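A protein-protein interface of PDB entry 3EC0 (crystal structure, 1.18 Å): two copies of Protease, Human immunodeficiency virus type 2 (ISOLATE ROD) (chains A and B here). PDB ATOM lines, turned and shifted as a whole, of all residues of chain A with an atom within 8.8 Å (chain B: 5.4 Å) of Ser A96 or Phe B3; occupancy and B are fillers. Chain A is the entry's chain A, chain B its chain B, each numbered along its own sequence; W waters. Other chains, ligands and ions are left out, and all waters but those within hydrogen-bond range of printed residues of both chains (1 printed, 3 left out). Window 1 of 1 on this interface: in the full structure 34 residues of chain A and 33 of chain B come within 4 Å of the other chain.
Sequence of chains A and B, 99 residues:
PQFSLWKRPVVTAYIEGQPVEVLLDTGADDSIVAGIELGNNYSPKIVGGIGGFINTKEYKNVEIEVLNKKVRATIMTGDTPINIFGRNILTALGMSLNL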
ATOM      1  N   PRO A   1     -13.297  25.524   3.397  1.00  0.00           N
ATOM      2  CA  PRO A   1     -14.094  24.317   3.558  1.00  0.00           C
ATOM      3  C   PRO A   1     -14.839  23.852   2.310  1.00  0.00           C
ATOM      4  O   PRO A   1     -15.282  24.654   1.479  1.00  0.00           O
ATOM      5  CB  PRO A   1     -15.202  24.752   4.544  1.00  0.00           C
ATOM      6  CG  PRO A   1     -15.348  26.209   4.207  1.00  0.00           C
ATOM      7  CD  PRO A   1     -13.891  26.656   4.155  1.00  0.00           C
ATOM      8  N   GLN A   2     -15.009  22.530   2.238  1.00  0.00           N
ATOM      9  CA  GLN A   2     -15.844  21.912   1.214  1.00  0.00           C
ATOM     10  C   GLN A   2     -16.880  21.018   1.894  1.00  0.00           C
ATOM     11  O   GLN A   2     -16.560  20.302   2.818  1.00  0.00           O
ATOM     12  CB  GLN A   2     -15.028  21.088   0.216  1.00  0.00           C
ATOM     13  CG  GLN A   2     -15.858  20.377  -0.849  1.00  0.00           C
ATOM     14  CD  GLN A   2     -15.083  19.854  -2.043  1.00  0.00           C
ATOM     15  OE1 GLN A   2     -14.417  20.586  -2.788  1.00  0.00           O
ATOM     16  NE2 GLN A   2     -15.175  18.548  -2.282  1.00  0.00           N
ATOM     17  N   PHE A   3     -18.107  21.070   1.407  1.00  0.00           N
ATOM     18  CA  PHE A   3     -19.190  20.196   1.849  1.00  0.00           C
ATOM     19  C   PHE A   3     -19.602  19.270   0.716  1.00  0.00           C
ATOM     20  O   PHE A   3     -20.111  19.735  -0.296  1.00  0.00           O
ATOM     21  CB  PHE A   3     -20.371  21.025   2.341  1.00  0.00           C
ATOM     22  CG  PHE A   3     -20.010  21.897   3.532  1.00  0.00           C
ATOM     23  CD1 PHE A   3     -19.432  23.153   3.408  1.00  0.00           C
ATOM     24  CD2 PHE A   3     -20.239  21.435   4.808  1.00  0.00           C
ATOM     25  CE1 PHE A   3     -19.075  23.884   4.529  1.00  0.00           C
ATOM     26  CE2 PHE A   3     -19.896  22.159   5.930  1.00  0.00           C
ATOM     27  CZ  PHE A   3     -19.315  23.386   5.802  1.00  0.00           C
ATOM     28  N   LEU A   5     -21.855  16.919   0.451  1.00  0.00           N
ATOM     29  CA  LEU A   5     -23.291  16.753   0.368  1.00  0.00           C
ATOM     30  C   LEU A   5     -23.671  15.291   0.463  1.00  0.00           C
ATOM     31  O   LEU A   5     -24.837  14.984   0.235  1.00  0.00           O
ATOM     32  CB  LEU A   5     -23.809  17.384  -0.924  1.00  0.00           C
ATOM     33  CG  LEU A   5     -23.432  18.827  -1.191  1.00  0.00           C
ATOM     34  CD1 LEU A   5     -23.958  19.310  -2.536  1.00  0.00           C
ATOM     35  CD2 LEU A   5     -23.952  19.773  -0.105  1.00  0.00           C
ATOM     36  N   THR A  26     -28.869  26.035   0.014  1.00  0.00           N
ATOM     37  CA  THR A  26     -28.959  26.795  -1.217  1.00  0.00           C
ATOM     38  C   THR A  26     -30.385  26.905  -1.710  1.00  0.00           C
ATOM     39  O   THR A  26     -30.659  27.721  -2.590  1.00  0.00           O
ATOM     40  CB  THR A  26     -28.095  26.150  -2.332  1.00  0.00           C
ATOM     41  OG1 THR A  26     -28.540  24.800  -2.553  1.00  0.00           O
ATOM     42  CG2 THR A  26     -26.627  26.099  -1.967  1.00  0.00           C
ATOM     43  N   ARG A  87     -29.454  31.686   1.349  1.00  0.00           N
ATOM     44  CA  ARG A  87     -28.536  32.368   0.466  1.00  0.00           C
ATOM     45  C   ARG A  87     -28.134  33.738   0.970  1.00  0.00           C
ATOM     46  O   ARG A  87     -27.021  34.194   0.623  1.00  0.00           O
ATOM     47  CB  ARG A  87     -29.133  32.432  -0.957  1.00  0.00           C
ATOM     48  CG  ARG A  87     -29.245  31.068  -1.641  1.00  0.00           C
ATOM     49  CD  ARG A  87     -29.670  31.215  -3.090  1.00  0.00           C
ATOM     50  NE  ARG A  87     -30.969  31.855  -3.207  1.00  0.00           N
ATOM     51  CZ  ARG A  87     -31.207  33.129  -3.519  1.00  0.00           C
ATOM     52  NH1 ARG A  87     -30.255  34.017  -3.793  1.00  0.00           N
ATOM     53  NH2 ARG A  87     -32.448  33.580  -3.589  1.00  0.00           N
ATOM     54  N   LEU A  90     -25.216  32.665   2.942  1.00  0.00           N
ATOM     55  CA  LEU A  90     -24.207  31.941   2.190  1.00  0.00           C
ATOM     56  C   LEU A  90     -23.439  32.916   1.315  1.00  0.00           C
ATOM     57  O   LEU A  90     -22.199  32.798   1.185  1.00  0.00           O
ATOM     58  CB  LEU A  90     -24.806  30.814   1.363  1.00  0.00           C
ATOM     59  CG  LEU A  90     -25.682  29.820   2.125  1.00  0.00           C
ATOM     60  CD1 LEU A  90     -26.141  28.721   1.177  1.00  0.00           C
ATOM     61  CD2 LEU A  90     -24.943  29.218   3.315  1.00  0.00           C
ATOM     62  N   THR A  91     -24.154  33.853   0.712  1.00  0.00           N
ATOM     63  CA  THR A  91     -23.451  34.838  -0.110  1.00  0.00           C
ATOM     64  C   THR A  91     -22.584  35.778   0.710  1.00  0.00           C
ATOM     65  O   THR A  91     -21.553  36.242   0.280  1.00  0.00           O
ATOM     66  CB  THR A  91     -24.412  35.724  -0.915  1.00  0.00           C
ATOM     67  OG1 THR A  91     -25.372  36.311  -0.041  1.00  0.00           O
ATOM     68  CG2 THR A  91     -25.151  34.930  -1.988  1.00  0.00           C
ATOM     69  N   LEU A  93     -20.939  34.997   3.231  1.00  0.00           N
ATOM     70  CA  LEU A  93     -19.769  34.220   3.589  1.00  0.00           C
ATOM     71  C   LEU A  93     -18.904  33.947   2.357  1.00  0.00           C
ATOM     72  O   LEU A  93     -17.789  33.506   2.614  1.00  0.00           O
ATOM     73  CB  LEU A  93     -20.117  32.851   4.181  1.00  0.00           C
ATOM     74  CG  LEU A  93     -20.964  32.842   5.435  1.00  0.00           C
ATOM     75  CD1 LEU A  93     -21.560  31.467   5.697  1.00  0.00           C
ATOM     76  CD2 LEU A  93     -20.120  33.265   6.626  1.00  0.00           C
ATOM     77  N   GLY A  94     -19.371  34.134   1.144  1.00  0.00           N
ATOM     78  CA  GLY A  94     -18.625  33.836  -0.071  1.00  0.00           C
ATOM     79  C   GLY A  94     -18.663  32.383  -0.493  1.00  0.00           C
ATOM     80  O   GLY A  94     -17.767  31.879  -1.173  1.00  0.00           O
ATOM     81  N   MET A  95     -19.734  31.687  -0.112  1.00  0.00           N
ATOM     82  CA  MET A  95     -19.963  30.314  -0.511  1.00  0.00           C
ATOM     83  C   MET A  95     -20.448  30.194  -1.941  1.00  0.00           C
ATOM     84  O   MET A  95     -21.153  31.075  -2.417  1.00  0.00           O
ATOM     85  CB  MET A  95     -21.074  29.675   0.334  1.00  0.00           C
ATOM     86  CG  MET A  95     -20.900  29.838   1.820  1.00  0.00           C
ATOM     87  SD  MET A  95     -21.295  28.336   2.707  1.00  0.00           S
ATOM     88  CE  MET A  95     -20.180  27.122   2.033  1.00  0.00           C
ATOM     89  N   SER A  96     -20.116  29.097  -2.602  1.00  0.00           N
ATOM     90  CA  SER A  96     -20.657  28.786  -3.916  1.00  0.00           C
ATOM     91  C   SER A  96     -21.024  27.300  -3.996  1.00  0.00           C
ATOM     92  O   SER A  96     -20.531  26.498  -3.216  1.00  0.00           O
ATOM     93  CB  SER A  96     -19.639  29.095  -5.018  1.00  0.00           C
ATOM     94  OG  SER A  96     -18.445  28.390  -4.783  1.00  0.00           O
ATOM     95  N   LEU A  97     -21.867  26.985  -4.946  1.00  0.00           N
ATOM     96  CA  LEU A  97     -22.328  25.642  -5.246  1.00  0.00           C
ATOM     97  C   LEU A  97     -21.706  25.316  -6.592  1.00  0.00           C
ATOM     98  O   LEU A  97     -21.862  26.079  -7.542  1.00  0.00           O
ATOM     99  CB  LEU A  97     -23.872  25.615  -5.154  1.00  0.00           C
ATOM    100  CG  LEU A  97     -24.461  24.289  -5.612  1.00  0.00           C
ATOM    101  CD1 LEU A  97     -24.151  23.187  -4.624  1.00  0.00           C
ATOM    102  CD2 LEU A  97     -25.957  24.525  -5.838  1.00  0.00           C
ATOM    103  N   ASN A  98     -20.945  24.241  -6.673  1.00  0.00           N
ATOM    104  CA  ASN A  98     -20.131  23.916  -7.829  1.00  0.00           C
ATOM    105  C   ASN A  98     -20.341  22.498  -8.353  1.00  0.00           C
ATOM    106  O   ASN A  98     -20.484  21.566  -7.590  1.00  0.00           O
ATOM    107  CB  ASN A  98     -18.657  24.080  -7.456  1.00  0.00           C
ATOM    108  CG  ASN A  98     -18.349  25.479  -7.014  1.00  0.00           C
ATOM    109  OD1 ASN A  98     -18.316  25.807  -5.832  1.00  0.00           O
ATOM    110  ND2 ASN A  98     -18.094  26.350  -7.993  1.00  0.00           N
ATOM    111  N   LEU A  99     -20.351  22.348  -9.672  1.00  0.00           N
ATOM    112  CA  LEU A  99     -20.236  21.115 -10.422  1.00  0.00           C
ATOM    113  C   LEU A  99     -18.943  21.111 -11.251  1.00  0.00           C
ATOM    114  O   LEU A  99     -18.841  21.937 -12.193  1.00  0.00           O
ATOM    115  CB  LEU A  99     -21.397  20.875 -11.366  1.00  0.00           C
ATOM    116  CG  LEU A  99     -21.486  19.512 -12.046  1.00  0.00           C
ATOM    117  CD1 LEU A  99     -20.858  18.424 -11.193  1.00  0.00           C
ATOM    118  CD2 LEU A  99     -22.928  19.138 -12.367  1.00  0.00           C
ATOM    119  OXT LEU A  99     -18.048  20.285 -10.968  1.00  0.00           O
ATOM    120  N   PRO B   1     -19.883  23.742 -13.814  1.00  0.00           N
ATOM    121  CA  PRO B   1     -20.644  24.968 -13.586  1.00  0.00           C
ATOM    122  C   PRO B   1     -20.543  25.444 -12.129  1.00  0.00           C
ATOM    123  O   PRO B   1     -20.351  24.660 -11.191  1.00  0.00           O
ATOM    124  CB  PRO B   1     -22.086  24.576 -13.894  1.00  0.00           C
ATOM    125  CG  PRO B   1     -22.059  23.184 -14.402  1.00  0.00           C
ATOM    126  CD  PRO B   1     -20.641  22.806 -14.686  1.00  0.00           C
ATOM    127  N   GLN B   2     -20.688  26.739 -11.933  1.00  0.00           N
ATOM    128  CA  GLN B   2     -20.709  27.483 -10.708  1.00  0.00           C
ATOM    129  C   GLN B   2     -21.954  28.353 -10.464  1.00  0.00           C
ATOM    130  O   GLN B   2     -22.423  29.158 -11.268  1.00  0.00           O
ATOM    131  CB  GLN B   2     -19.501  28.443 -10.695  1.00  0.00           C
ATOM    132  CG  GLN B   2     -19.359  29.204  -9.384  1.00  0.00           C
ATOM    133  CD  GLN B   2     -17.907  29.402  -8.988  1.00  0.00           C
ATOM    134  OE1 GLN B   2     -17.563  29.450  -7.814  1.00  0.00           O
ATOM    135  NE2 GLN B   2     -17.019  29.519  -9.973  1.00  0.00           N
ATOM    136  N   PHE B   3     -22.496  28.182  -9.252  1.00  0.00           N
ATOM    137  CA  PHE B   3     -23.628  28.932  -8.746  1.00  0.00           C
ATOM    138  C   PHE B   3     -23.163  29.803  -7.594  1.00  0.00           C
ATOM    139  O   PHE B   3     -22.825  29.278  -6.518  1.00  0.00           O
ATOM    140  CB  PHE B   3     -24.745  27.962  -8.329  1.00  0.00           C
ATOM    141  CG  PHE B   3     -25.278  27.185  -9.512  1.00  0.00           C
ATOM    142  CD1 PHE B   3     -24.714  25.977  -9.851  1.00  0.00           C
ATOM    143  CD2 PHE B   3     -26.306  27.651 -10.312  1.00  0.00           C
ATOM    144  CE1 PHE B   3     -25.151  25.259 -10.936  1.00  0.00           C
ATOM    145  CE2 PHE B   3     -26.755  26.937 -11.392  1.00  0.00           C
ATOM    146  CZ  PHE B   3     -26.170  25.722 -11.721  1.00  0.00           C
ATOM    147  N   SER B   4     -23.115  31.121  -7.812  1.00  0.00           N
ATOM    148  CA  SER B   4     -22.588  32.045  -6.798  1.00  0.00           C
ATOM    149  C   SER B   4     -23.599  32.440  -5.725  1.00  0.00           C
ATOM    150  O   SER B   4     -23.264  33.091  -4.750  1.00  0.00           O
ATOM    151  CB  SER B   4     -22.070  33.300  -7.499  1.00  0.00           C
ATOM    152  OG  SER B   4     -20.798  32.935  -8.072  1.00  0.00           O
ATOM    153  N   LEU B   5     -24.843  32.022  -5.876  1.00  0.00           N
ATOM    154  CA  LEU B   5     -25.910  32.076  -4.865  1.00  0.00           C
ATOM    155  C   LEU B   5     -26.508  33.447  -4.607  1.00  0.00           C
ATOM    156  O   LEU B   5     -27.395  33.572  -3.755  1.00  0.00           O
ATOM    157  CB  LEU B   5     -25.457  31.403  -3.551  1.00  0.00           C
ATOM    158  CG  LEU B   5     -25.003  29.944  -3.719  1.00  0.00           C
ATOM    159  CD1 LEU B   5     -24.513  29.420  -2.373  1.00  0.00           C
ATOM    160  CD2 LEU B   5     -26.066  29.021  -4.281  1.00  0.00           C
ATOM    161  N   LYS B   7     -28.345  34.719  -6.842  1.00  0.00           N
ATOM    162  CA  LYS B   7     -29.655  34.363  -7.359  1.00  0.00           C
ATOM    163  C   LYS B   7     -29.899  32.904  -6.983  1.00  0.00           C
ATOM    164  O   LYS B   7     -28.976  32.152  -6.657  1.00  0.00           O
ATOM    165  CB  LYS B   7     -29.778  34.570  -8.856  1.00  0.00           C
ATOM    166  CG  LYS B   7     -28.794  33.823  -9.720  1.00  0.00           C
ATOM    167  CD  LYS B   7     -28.831  34.369 -11.140  1.00  0.00           C
ATOM    168  CE  LYS B   7     -28.107  33.474 -12.113  1.00  0.00           C
ATOM    169  NZ  LYS B   7     -27.948  32.074 -11.632  1.00  0.00           N
ATOM    170  N   PRO B   9     -30.205  29.096  -7.314  1.00  0.00           N
ATOM    171  CA  PRO B   9     -29.569  28.157  -8.270  1.00  0.00           C
ATOM    172  C   PRO B   9     -30.609  27.264  -8.915  1.00  0.00           C
ATOM    173  O   PRO B   9     -30.778  26.078  -8.645  1.00  0.00           O
ATOM    174  CB  PRO B   9     -28.631  27.349  -7.365  1.00  0.00           C
ATOM    175  CG  PRO B   9     -29.293  27.337  -6.033  1.00  0.00           C
ATOM    176  CD  PRO B   9     -29.992  28.681  -5.914  1.00  0.00           C
ATOM    177  N   VAL B  10     -31.323  27.905  -9.851  1.00  0.00           N
ATOM    178  CA  VAL B  10     -32.355  27.238 -10.629  1.00  0.00           C
ATOM    179  C   VAL B  10     -31.849  26.907 -12.008  1.00  0.00           C
ATOM    180  O   VAL B  10     -31.226  27.741 -12.634  1.00  0.00           O
ATOM    181  CB  VAL B  10     -33.579  28.164 -10.700  1.00  0.00           C
ATOM    182  CG1 VAL B  10     -34.574  27.695 -11.731  1.00  0.00           C
ATOM    183  CG2 VAL B  10     -34.192  28.268  -9.317  1.00  0.00           C
ATOM    184  N   VAL B  11     -32.204  25.726 -12.482  1.00  0.00           N
ATOM    185  CA  VAL B  11     -31.858  25.257 -13.801  1.00  0.00           C
ATOM    186  C   VAL B  11     -33.048  24.547 -14.396  1.00  0.00           C
ATOM    187  O   VAL B  11     -34.001  24.167 -13.732  1.00  0.00           O
ATOM    188  CB  VAL B  11     -30.628  24.303 -13.822  1.00  0.00           C
ATOM    189  CG1 VAL B  11     -29.362  24.990 -13.355  1.00  0.00           C
ATOM    190  CG2 VAL B  11     -30.914  23.055 -13.026  1.00  0.00           C
ATOM    191  N   LEU B  24     -31.595  23.671  -7.169  1.00  0.00           N
ATOM    192  CA  LEU B  24     -30.548  22.848  -6.604  1.00  0.00           C
ATOM    193  C   LEU B  24     -30.484  23.171  -5.106  1.00  0.00           C
ATOM    194  O   LEU B  24     -30.156  24.290  -4.717  1.00  0.00           O
ATOM    195  CB  LEU B  24     -29.245  23.142  -7.324  1.00  0.00           C
ATOM    196  CG  LEU B  24     -29.308  22.923  -8.841  1.00  0.00           C
ATOM    197  CD1 LEU B  24     -27.946  23.297  -9.425  1.00  0.00           C
ATOM    198  CD2 LEU B  24     -29.727  21.504  -9.218  1.00  0.00           C
ATOM    199  N   LEU B  67     -27.729  19.858 -16.290  1.00  0.00           N
ATOM    200  CA  LEU B  67     -26.359  20.340 -16.325  1.00  0.00           C
ATOM    201  C   LEU B  67     -25.443  19.528 -17.218  1.00  0.00           C
ATOM    202  O   LEU B  67     -24.287  19.233 -16.933  1.00  0.00           O
ATOM    203  CB  LEU B  67     -25.818  20.404 -14.896  1.00  0.00           C
ATOM    204  CG  LEU B  67     -26.462  21.477 -14.011  1.00  0.00           C
ATOM    205  CD1 LEU B  67     -25.901  21.401 -12.606  1.00  0.00           C
ATOM    206  CD2 LEU B  67     -26.293  22.881 -14.571  1.00  0.00           C
ATOM    207  N   MET B  95     -21.634  17.322  -7.152  1.00  0.00           N
ATOM    208  CA  MET B  95     -21.592  18.706  -6.738  1.00  0.00           C
ATOM    209  C   MET B  95     -21.144  18.848  -5.289  1.00  0.00           C
ATOM    210  O   MET B  95     -21.195  17.866  -4.549  1.00  0.00           O
ATOM    211  CB  MET B  95     -22.957  19.383  -6.909  1.00  0.00           C
ATOM    212  CG  MET B  95     -23.471  19.372  -8.335  1.00  0.00           C
ATOM    213  SD  MET B  95     -24.922  20.416  -8.539  1.00  0.00           S
ATOM    214  CE  MET B  95     -24.211  22.055  -8.529  1.00  0.00           C
ATOM    215  N   SER B  96     -20.725  20.056  -4.959  1.00  0.00           N
ATOM    216  CA  SER B  96     -20.260  20.442  -3.642  1.00  0.00           C
ATOM    217  C   SER B  96     -20.537  21.907  -3.323  1.00  0.00           C
ATOM    218  O   SER B  96     -20.722  22.719  -4.234  1.00  0.00           O
ATOM    219  CB  SER B  96     -18.754  20.163  -3.508  1.00  0.00           C
ATOM    220  OG  SER B  96     -17.990  20.965  -4.382  1.00  0.00           O
ATOM    221  N   LEU B  97     -20.570  22.234  -2.027  1.00  0.00           N
ATOM    222  CA  LEU B  97     -20.650  23.575  -1.454  1.00  0.00           C
ATOM    223  C   LEU B  97     -19.236  23.944  -0.962  1.00  0.00           C
ATOM    224  O   LEU B  97     -18.620  23.130  -0.263  1.00  0.00           O
ATOM    225  CB  LEU B  97     -21.628  23.595  -0.315  1.00  0.00           C
ATOM    226  CG  LEU B  97     -22.445  24.749   0.158  1.00  0.00           C
ATOM    227  CD1 LEU B  97     -23.102  25.485  -0.996  1.00  0.00           C
ATOM    228  CD2 LEU B  97     -23.440  24.186   1.192  1.00  0.00           C
ATOM    229  N   ASN B  98     -18.795  25.134  -1.369  1.00  0.00           N
ATOM    230  CA  ASN B  98     -17.432  25.584  -1.140  1.00  0.00           C
ATOM    231  C   ASN B  98     -17.331  27.021  -0.634  1.00  0.00           C
ATOM    232  O   ASN B  98     -18.123  27.909  -1.003  1.00  0.00           O
ATOM    233  CB  ASN B  98     -16.667  25.437  -2.459  1.00  0.00           C
ATOM    234  CG  ASN B  98     -16.607  23.998  -2.950  1.00  0.00           C
ATOM    235  OD1 ASN B  98     -17.459  23.488  -3.664  1.00  0.00           O
ATOM    236  ND2 ASN B  98     -15.550  23.293  -2.576  1.00  0.00           N
ATOM    237  N   LEU B  99     -16.359  27.255   0.222  1.00  0.00           N
ATOM    238  CA  LEU B  99     -15.992  28.554   0.751  1.00  0.00           C
ATOM    239  C   LEU B  99     -14.481  28.750   0.721  1.00  0.00           C
ATOM    240  O   LEU B  99     -13.789  27.785   1.132  1.00  0.00           O
ATOM    241  CB  LEU B  99     -16.478  28.614   2.187  1.00  0.00           C
ATOM    242  CG  LEU B  99     -17.015  29.919   2.729  1.00  0.00           C
ATOM    243  CD1 LEU B  99     -17.006  29.838   4.248  1.00  0.00           C
ATOM    244  CD2 LEU B  99     -16.250  31.101   2.194  1.00  0.00           C
ATOM    245  OXT LEU B  99     -14.000  29.842   0.344  1.00  0.00           O
HETATM  246  O   HOH W   1     -14.715  31.891  -1.335  1.00  0.00           O
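The backbone carbonyl oxygen of Pro A1 lies within hydrogen-bond range of the backbone NH of Leu B99 (3.1 Å). The side-chain amide oxygen (OE1) of Gln A2 is in hydrogen-bond range of the side-chain amide nitrogen (ND2) of Asn B98 (2.9 Å). The backbone carbonyl oxygen of Leu B97 lies within hydrogen-bond range of the backbone NH of Phe A3 (2.7 Å). The side-chain hydroxyl (OG1) of Thr A26 sits at hydrogen-bond distance from the backbone carbonyl oxygen (O) of Leu B24, 2.7 Å away. NH1 of Arg A87 lies within hydrogen-bond range of O of Leu B5, at 2.9 Å. The side-chain hydroxyl (OG) of Ser A96 sits at hydrogen-bond distance from the side-chain amide oxygen (OE1) of Gln B2, at 3.3 Å. The backbone carbonyl oxygen (O) of Asn B98 is in hydrogen-bond range of the backbone NH (N) of Ser A96. The backbone carbonyl oxygen (O) of Leu A97 is in hydrogen-bond range of the backbone NH (N) of Phe B3 (2.8 Å). ND2 of Asn A98 is in hydrogen-bond range of OE1 of Gln B2 (3.2 Å). The backbone NH (N) of Asn A98 is in hydrogen-bond range of the backbone carbonyl oxygen (O) of Ser B96, at 2.9 Å. The side-chain amide oxygen (OD1) of Asn A98 sits close to the side-chain amide oxygen (OD1) of Asn B98 (3.3 Å). N of Leu A99 sits at hydrogen-bond distance from O of Pro B1 (2.8 Å).
The side-chain hydroxyl of Thr A91 lies within hydrogen-bond range of the backbone carbonyl oxygen of Arg A87 (2.8 Å). O of Leu A90 sits at hydrogen-bond distance from N of Met A95 (3.0 Å). The side-chain hydroxyl (OG) of Ser A96 sits at hydrogen-bond distance from the side-chain amide oxygen (OD1) of Asn A98, 2.8 Å away. The backbone NH (N) of Leu B24 sits at hydrogen-bond distance from the backbone carbonyl oxygen (O) of Pro B9 (2.9 Å). The side-chain hydroxyl of Ser B96 lies within hydrogen-bond range of the side-chain amide oxygen of Asn B98 (2.7 Å).
CD2 of Leu B5 touches CG2 of Thr A26, 3.8 Å away. Pro B9 touches Thr A26. Thr A26 touches Leu B97 (CG2 to CD1, 3.7 Å). CG2 of Thr A91 touches O of Ser B4 (3.8 Å). O of Leu A93 touches CD2 of Leu B99 (2.9 Å). O of Gly A94 touches O of Asn B98 (3.99 Å). O of Gly A94 touches CD2 of Leu B99, 3.8 Å away. Met A95 touches Leu B99. Met B95 touches Asn A98 (CA to O, 3.2 Å). CG of Met B95 touches CB of Leu A99, 3.97 Å away.
Printed residues of chain B within 4 Å of Leu A90: Leu B5 (3.97 Å). Of chain B, only Gln B2, Phe B3, Ser B96, Leu B97 and Asn B98 come within 4 Å of Ser A96. Of the printed residues of chain B, Asn A98 touches Pro B1 (3.5 Å), Gln B2 (3.2 Å), Met B95 (3.2 Å), Ser B96 (2.9 Å) and Asn B98 (3.3 Å). Phe B3 touches two residues of chain A. Printed residues of chain A within 4 Å of Asn B98: Pro A1 (3.5 Å), Gln A2 (2.9 Å), Gly A94 (3.99 Å), Met A95 (3.1 Å), Ser A96 (2.8 Å) and Asn A98 (3.3 Å). The nearest residue of chain B that does not touch Ser A96 is Leu B5 (4.2 Å).
Printed residues of chain A that touch a printed residue of chain B: Pro A1, Gln A2, Phe A3, Leu A5, Thr A26, Arg A87, Leu A90, Thr A91, Leu A93, Gly A94, Met A95, Ser A96, Leu A97, Asn A98 and Leu A99. Of the 16 printed residues of chain B, 14 touch a printed residue of chain A. Hydrophobic or aromatic side chains of chain B that line the printed part of chain A: Pro B1, Phe B3, Leu B5, Pro B9, Leu B24, Leu B67, Met B95, Leu B97 and Leu B99. Among the printed residues, 44 pairs touch across the chains.
Gln A2 touches Ser B96, and with the chains exchanged Ser A96 touches Gln B2. Gln A2 touches Asn B98, and with the chains exchanged Asn A98 touches Gln B2. Ser A96 touches Asn B98, and with the chains exchanged Asn A98 touches Ser B96. Asn A98 touches its own counterpart, Asn B98. Positions printed for both chains: 1, 2, 3, 5, 95, 96, 97, 98 and 99. Of the 44 pairs that touch across the chains among the printed residues, 28 have their exchanged pair printed and touching as well.
Water W1 bridges OXT of Leu B99 and O of Gly A94.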
